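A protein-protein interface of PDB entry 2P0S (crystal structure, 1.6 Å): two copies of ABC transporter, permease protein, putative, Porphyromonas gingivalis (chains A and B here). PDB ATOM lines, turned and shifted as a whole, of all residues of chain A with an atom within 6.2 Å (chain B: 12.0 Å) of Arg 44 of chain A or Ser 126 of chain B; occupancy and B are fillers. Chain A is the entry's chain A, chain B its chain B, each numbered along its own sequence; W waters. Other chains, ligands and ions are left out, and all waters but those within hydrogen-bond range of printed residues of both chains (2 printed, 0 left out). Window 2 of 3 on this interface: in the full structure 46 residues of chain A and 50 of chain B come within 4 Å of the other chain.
Arg 44 of chain A touches just these residues of chain B: Trp 125, Ser 126 and Asp 128. Of the printed residues of chain A, Ser 126 of chain B touches Arg 44 (3.1 Å). Ala 40 of chain A touches just one residue of chain B: Trp 125. No residue of chain B comes within 4 Å of Glu 41 of chain A. Of the printed residues of chain B, Lys 45 of chain A touches Asp 128. Tyr 75 of chain A touches two residues of chain B. Of the printed residues of chain A, Asp 128 of chain B touches Arg 44 (3.3 Å) and Lys 45 (3.6 Å). Of the printed residues of chain A, Lys 124 of chain B touches Tyr 75. Thr 122 of chain B touches none of the printed residues of chain A. Gly 129 of chain B touches none of the printed residues of chain A. The nearest residue of chain B that does not touch Arg 44 of chain A is Glu 127 of chain B (4.1 Å). The nearest residue of chain A that does not touch Ser 126 of chain B is Glu 41 of chain A (5.9 Å).
O of Ser 126 of chain B lies within hydrogen-bond range of NH1 of Arg 44 of chain A (3.1 Å).
Printed residues of chain A that touch a printed residue of chain B: Ala 40, Arg 44, Lys 45 and Tyr 75. Printed residues of chain B that touch a printed residue of chain A: Lys 124, Trp 125, Ser 126 and Asp 128. Hydrophobic or aromatic side chains of chain B that line the printed part of chain A: Trp 125.
Water W2 lies within hydrogen-bond range of OG of Ser 126 of chain B (2.6 Å), NH1 of Arg 44 of chain A (3.2 Å) and O of Glu 127 of chain B (3.4 Å). Water W1 lies within hydrogen-bond range of O of Arg 44 of chain A (2.9 Å) and OD1 of Asp 128 of chain B (3.3 Å).
The guanidinium group of Arg 44 of chain A lies within salt-bridge range of the side-chain carboxylate of Glu 41 of chain A (2.5 Å). The side-chain carboxylate (OE2) of Glu 41 of chain A is in salt-bridge range of the side-chain amino group (NZ) of Lys 45 of chain A, at 3.9 Å. OH of Tyr 75 of chain A sits at hydrogen-bond distance from O of Tyr 43 of chain A, 2.5 Å away. The side-chain amino group (NZ) of Lys 124 of chain B lies within salt-bridge range of the side-chain carboxylate (OE2) of Glu 127 of chain B, 3.2 Å away.
No position is printed for both chains. Of the 7 pairs that touch across the chains among the printed residues, none has its exchanged pair printed and touching as well.
Among the printed residues, pairs that only touch across the chains: Ala 40 of chain A with Trp 125 of chain B (3.3 Å), Arg 44 of chain A with Trp 125 of chain B (3.5 Å), Arg 44 of chain A with Asp 128 of chain B (3.3 Å), Lys 45 of chain A with Asp 128 of chain B (3.6 Å), Tyr 75 of chain A with Lys 124 of chain B (3.2 Å) and Tyr 75 of chain A with Trp 125 of chain B (3.5 Å).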
ATOM      1  N   THR A  39      -0.974 -14.884  25.792  1.00  0.00           N
ATOM      2  CA  THR A  39      -0.405 -16.188  25.986  1.00  0.00           C
ATOM      3  C   THR A  39       1.075 -16.166  25.773  1.00  0.00           C
ATOM      4  O   THR A  39       1.631 -15.195  25.136  1.00  0.00           O
ATOM      5  CB  THR A  39      -0.972 -17.212  24.963  1.00  0.00           C
ATOM      6  OG1 THR A  39      -0.559 -16.858  23.629  1.00  0.00           O
ATOM      7  CG2 THR A  39      -2.498 -17.221  25.028  1.00  0.00           C
ATOM      8  N   ALA A  40       1.735 -17.228  26.263  1.00  0.00           N
ATOM      9  CA  ALA A  40       3.139 -17.392  25.980  1.00  0.00           C
ATOM     10  C   ALA A  40       3.447 -17.314  24.467  1.00  0.00           C
ATOM     11  O   ALA A  40       4.441 -16.689  24.095  1.00  0.00           O
ATOM     12  CB  ALA A  40       3.657 -18.728  26.590  1.00  0.00           C
ATOM     13  N   GLU A  41       2.675 -18.024  23.627  1.00  0.00           N
ATOM     14  CA  GLU A  41       2.889 -18.039  22.174  1.00  0.00           C
ATOM     15  C   GLU A  41       2.656 -16.636  21.611  1.00  0.00           C
ATOM     16  O   GLU A  41       3.390 -16.167  20.734  1.00  0.00           O
ATOM     17  CB  GLU A  41       1.936 -19.034  21.476  1.00  0.00           C
ATOM     18  CG  GLU A  41       1.983 -19.032  19.887  1.00  0.00           C
ATOM     19  CD  GLU A  41       3.400 -19.355  19.280  1.00  0.00           C
ATOM     20  OE1 GLU A  41       4.268 -19.933  19.974  1.00  0.00           O
ATOM     21  OE2 GLU A  41       3.651 -18.981  18.102  1.00  0.00           O
ATOM     22  N   GLU A  42       1.657 -15.932  22.091  1.00  0.00           N
ATOM     23  CA  GLU A  42       1.570 -14.539  21.574  1.00  0.00           C
ATOM     24  C   GLU A  42       2.695 -13.648  21.935  1.00  0.00           C
ATOM     25  O   GLU A  42       3.082 -12.819  21.062  1.00  0.00           O
ATOM     26  CB  GLU A  42       0.264 -13.910  21.997  1.00  0.00           C
ATOM     27  CG  GLU A  42      -0.885 -14.675  21.484  1.00  0.00           C
ATOM     28  CD  GLU A  42      -2.131 -14.086  22.003  1.00  0.00           C
ATOM     29  OE1 GLU A  42      -2.267 -14.044  23.247  1.00  0.00           O
ATOM     30  OE2 GLU A  42      -2.934 -13.594  21.179  1.00  0.00           O
ATOM     31  N   TYR A  43       3.155 -13.663  23.197  1.00  0.00           N
ATOM     32  CA  TYR A  43       4.333 -12.924  23.575  1.00  0.00           C
ATOM     33  C   TYR A  43       5.563 -13.358  22.713  1.00  0.00           C
ATOM     34  O   TYR A  43       6.385 -12.519  22.304  1.00  0.00           O
ATOM     35  CB  TYR A  43       4.641 -13.088  25.075  1.00  0.00           C
ATOM     36  CG  TYR A  43       3.748 -12.355  25.998  1.00  0.00           C
ATOM     37  CD1 TYR A  43       3.627 -10.970  25.923  1.00  0.00           C
ATOM     38  CD2 TYR A  43       3.080 -13.037  27.079  1.00  0.00           C
ATOM     39  CE1 TYR A  43       2.837 -10.270  26.824  1.00  0.00           C
ATOM     40  CE2 TYR A  43       2.299 -12.320  28.014  1.00  0.00           C
ATOM     41  CZ  TYR A  43       2.190 -10.916  27.837  1.00  0.00           C
ATOM     42  OH  TYR A  43       1.479 -10.134  28.714  1.00  0.00           O
ATOM     43  N   ARG A  44       5.695 -14.645  22.424  1.00  0.00           N
ATOM     44  CA  ARG A  44       6.781 -15.072  21.583  1.00  0.00           C
ATOM     45  C   ARG A  44       6.746 -14.357  20.229  1.00  0.00           C
ATOM     46  O   ARG A  44       7.757 -13.929  19.770  1.00  0.00           O
ATOM     47  CB  ARG A  44       6.696 -16.565  21.251  1.00  0.00           C
ATOM     48  CG  ARG A  44       7.960 -17.139  20.556  1.00  0.00           C
ATOM     49  CD  ARG A  44       7.826 -18.738  20.347  1.00  0.00           C
ATOM     50  NE  ARG A  44       6.759 -18.946  19.355  1.00  0.00           N
ATOM     51  CZ  ARG A  44       6.981 -18.819  18.012  1.00  0.00           C
ATOM     52  NH1 ARG A  44       8.214 -18.585  17.555  1.00  0.00           N
ATOM     53  NH2 ARG A  44       5.994 -18.953  17.129  1.00  0.00           N
ATOM     54  N   LYS A  45       5.593 -14.411  19.580  1.00  0.00           N
ATOM     55  CA  LYS A  45       5.449 -13.895  18.215  1.00  0.00           C
ATOM     56  C   LYS A  45       5.707 -12.377  18.182  1.00  0.00           C
ATOM     57  O   LYS A  45       6.323 -11.864  17.203  1.00  0.00           O
ATOM     58  CB  LYS A  45       4.045 -14.213  17.688  1.00  0.00           C
ATOM     59  CG  LYS A  45       3.727 -15.784  17.556  1.00  0.00           C
ATOM     60  CD  LYS A  45       2.238 -16.036  17.051  1.00  0.00           C
ATOM     61  CE  LYS A  45       1.960 -17.432  16.350  1.00  0.00           C
ATOM     62  NZ  LYS A  45       2.101 -17.575  14.812  1.00  0.00           N
ATOM     63  N   MET A  46       5.275 -11.652  19.214  1.00  0.00           N
ATOM     64  CA  MET A  46       5.284 -10.194  19.126  1.00  0.00           C
ATOM     65  C   MET A  46       6.714  -9.718  19.380  1.00  0.00           C
ATOM     66  O   MET A  46       7.164  -8.648  18.900  1.00  0.00           O
ATOM     67  CB  MET A  46       4.206  -9.587  20.008  1.00  0.00           C
ATOM     68  CG  MET A  46       4.647  -9.193  21.326  1.00  0.00           C
ATOM     69  SD  MET A  46       3.207  -8.577  22.482  1.00  0.00           S
ATOM     70  CE  MET A  46       2.883  -6.809  21.769  1.00  0.00           C
ATOM     71  N   GLY A  47       7.498 -10.584  19.997  1.00  0.00           N
ATOM     72  CA  GLY A  47       8.898 -10.288  20.302  1.00  0.00           C
ATOM     73  C   GLY A  47       9.167  -9.304  21.446  1.00  0.00           C
ATOM     74  O   GLY A  47       8.246  -8.584  21.916  1.00  0.00           O
ATOM     75  N   ALA A  48      10.446  -9.254  21.884  1.00  0.00           N
ATOM     76  CA  ALA A  48      10.787  -8.596  23.126  1.00  0.00           C
ATOM     77  C   ALA A  48      10.482  -7.087  23.025  1.00  0.00           C
ATOM     78  O   ALA A  48       9.939  -6.465  23.934  1.00  0.00           O
ATOM     79  CB  ALA A  48      12.262  -8.837  23.436  1.00  0.00           C
ATOM     80  N   TYR A  75      12.830 -14.997  25.750  1.00  0.00           N
ATOM     81  CA  TYR A  75      13.413 -14.678  24.405  1.00  0.00           C
ATOM     82  C   TYR A  75      14.909 -15.065  24.306  1.00  0.00           C
ATOM     83  O   TYR A  75      15.365 -15.560  23.210  1.00  0.00           O
ATOM     84  CB  TYR A  75      13.257 -13.119  24.178  1.00  0.00           C
ATOM     85  CG  TYR A  75      11.838 -12.737  24.161  1.00  0.00           C
ATOM     86  CD1 TYR A  75      11.005 -13.061  23.073  1.00  0.00           C
ATOM     87  CD2 TYR A  75      11.307 -11.995  25.223  1.00  0.00           C
ATOM     88  CE1 TYR A  75       9.713 -12.730  23.038  1.00  0.00           C
ATOM     89  CE2 TYR A  75       9.958 -11.541  25.168  1.00  0.00           C
ATOM     90  CZ  TYR A  75       9.162 -11.936  24.100  1.00  0.00           C
ATOM     91  OH  TYR A  75       7.831 -11.482  24.011  1.00  0.00           O
ATOM     92  N   THR B 122      13.322 -24.332  32.298  1.00  0.00           N
ATOM     93  CA  THR B 122      13.380 -23.029  31.636  1.00  0.00           C
ATOM     94  C   THR B 122      13.844 -23.278  30.202  1.00  0.00           C
ATOM     95  O   THR B 122      14.784 -24.099  29.960  1.00  0.00           O
ATOM     96  CB  THR B 122      14.342 -22.144  32.365  1.00  0.00           C
ATOM     97  OG1 THR B 122      13.922 -22.007  33.718  1.00  0.00           O
ATOM     98  CG2 THR B 122      14.451 -20.829  31.763  1.00  0.00           C
ATOM     99  N   TYR B 123      13.227 -22.578  29.247  1.00  0.00           N
ATOM    100  CA  TYR B 123      13.494 -22.837  27.845  1.00  0.00           C
ATOM    101  C   TYR B 123      13.710 -21.456  27.216  1.00  0.00           C
ATOM    102  O   TYR B 123      13.141 -20.468  27.675  1.00  0.00           O
ATOM    103  CB  TYR B 123      12.286 -23.412  27.184  1.00  0.00           C
ATOM    104  CG  TYR B 123      11.834 -24.746  27.801  1.00  0.00           C
ATOM    105  CD1 TYR B 123      12.589 -25.988  27.621  1.00  0.00           C
ATOM    106  CD2 TYR B 123      10.727 -24.803  28.603  1.00  0.00           C
ATOM    107  CE1 TYR B 123      12.255 -27.222  28.195  1.00  0.00           C
ATOM    108  CE2 TYR B 123      10.341 -26.096  29.166  1.00  0.00           C
ATOM    109  CZ  TYR B 123      11.097 -27.280  28.965  1.00  0.00           C
ATOM    110  OH  TYR B 123      10.614 -28.457  29.494  1.00  0.00           O
ATOM    111  N   LYS B 124      14.361 -21.498  26.077  1.00  0.00           N
ATOM    112  CA  LYS B 124      14.420 -20.316  25.212  1.00  0.00           C
ATOM    113  C   LYS B 124      13.346 -20.590  24.095  1.00  0.00           C
ATOM    114  O   LYS B 124      13.300 -21.690  23.464  1.00  0.00           O
ATOM    115  CB  LYS B 124      15.774 -20.333  24.553  1.00  0.00           C
ATOM    116  CG  LYS B 124      15.954 -19.148  23.656  1.00  0.00           C
ATOM    117  CD  LYS B 124      17.401 -19.022  23.008  1.00  0.00           C
ATOM    118  CE  LYS B 124      17.297 -17.793  22.109  1.00  0.00           C
ATOM    119  NZ  LYS B 124      18.660 -17.607  21.570  1.00  0.00           N
ATOM    120  N   TRP B 125      12.399 -19.694  23.869  1.00  0.00           N
ATOM    121  CA  TRP B 125      11.409 -19.898  22.839  1.00  0.00           C
ATOM    122  C   TRP B 125      12.085 -20.107  21.469  1.00  0.00           C
ATOM    123  O   TRP B 125      13.164 -19.514  21.192  1.00  0.00           O
ATOM    124  CB  TRP B 125      10.598 -18.613  22.727  1.00  0.00           C
ATOM    125  CG  TRP B 125       9.432 -18.472  23.635  1.00  0.00           C
ATOM    126  CD1 TRP B 125       8.395 -19.315  23.740  1.00  0.00           C
ATOM    127  CD2 TRP B 125       9.044 -17.273  24.327  1.00  0.00           C
ATOM    128  NE1 TRP B 125       7.422 -18.772  24.552  1.00  0.00           N
ATOM    129  CE2 TRP B 125       7.835 -17.551  24.997  1.00  0.00           C
ATOM    130  CE3 TRP B 125       9.698 -16.069  24.591  1.00  0.00           C
ATOM    131  CZ2 TRP B 125       7.197 -16.632  25.848  1.00  0.00           C
ATOM    132  CZ3 TRP B 125       9.072 -15.132  25.453  1.00  0.00           C
ATOM    133  CH2 TRP B 125       7.821 -15.401  25.998  1.00  0.00           C
ATOM    134  N   SER B 126      11.374 -20.818  20.579  1.00  0.00           N
ATOM    135  CA  SER B 126      11.910 -21.024  19.228  1.00  0.00           C
ATOM    136  C   SER B 126      11.864 -19.653  18.568  1.00  0.00           C
ATOM    137  O   SER B 126      11.009 -18.774  18.913  1.00  0.00           O
ATOM    138  CB  SER B 126      11.058 -22.066  18.497  1.00  0.00           C
ATOM    139  OG  SER B 126       9.702 -21.607  18.447  1.00  0.00           O
ATOM    140  N   GLU B 127      12.766 -19.478  17.618  1.00  0.00           N
ATOM    141  CA  GLU B 127      12.912 -18.121  17.056  1.00  0.00           C
ATOM    142  C   GLU B 127      11.913 -17.869  15.981  1.00  0.00           C
ATOM    143  O   GLU B 127      11.520 -18.711  15.213  1.00  0.00           O
ATOM    144  CB  GLU B 127      14.351 -17.836  16.611  1.00  0.00           C
ATOM    145  CG  GLU B 127      15.310 -17.580  17.880  1.00  0.00           C
ATOM    146  CD  GLU B 127      16.795 -17.674  17.596  1.00  0.00           C
ATOM    147  OE1 GLU B 127      17.169 -17.807  16.412  1.00  0.00           O
ATOM    148  OE2 GLU B 127      17.621 -17.582  18.554  1.00  0.00           O
ATOM    149  N   ASP B 128      11.439 -16.634  15.913  1.00  0.00           N
ATOM    150  CA  ASP B 128      10.383 -16.434  14.960  1.00  0.00           C
ATOM    151  C   ASP B 128      10.935 -15.491  13.907  1.00  0.00           C
ATOM    152  O   ASP B 128      10.354 -15.400  12.850  1.00  0.00           O
ATOM    153  CB  ASP B 128       9.016 -16.050  15.604  1.00  0.00           C
ATOM    154  CG  ASP B 128       8.719 -14.575  15.598  1.00  0.00           C
ATOM    155  OD1 ASP B 128       9.279 -13.837  16.469  1.00  0.00           O
ATOM    156  OD2 ASP B 128       7.875 -14.146  14.740  1.00  0.00           O
ATOM    157  N   GLY B 129      12.065 -14.853  14.212  1.00  0.00           N
ATOM    158  CA  GLY B 129      12.608 -13.760  13.395  1.00  0.00           C
ATOM    159  C   GLY B 129      13.321 -14.197  12.133  1.00  0.00           C
ATOM    160  O   GLY B 129      14.276 -13.535  11.717  1.00  0.00           O
HETATM  161  O   HOH W   1      10.657 -13.883  19.452  1.00  0.00           O
HETATM  162  O   HOH W   2       9.220 -21.182  15.910  1.00  0.00           O
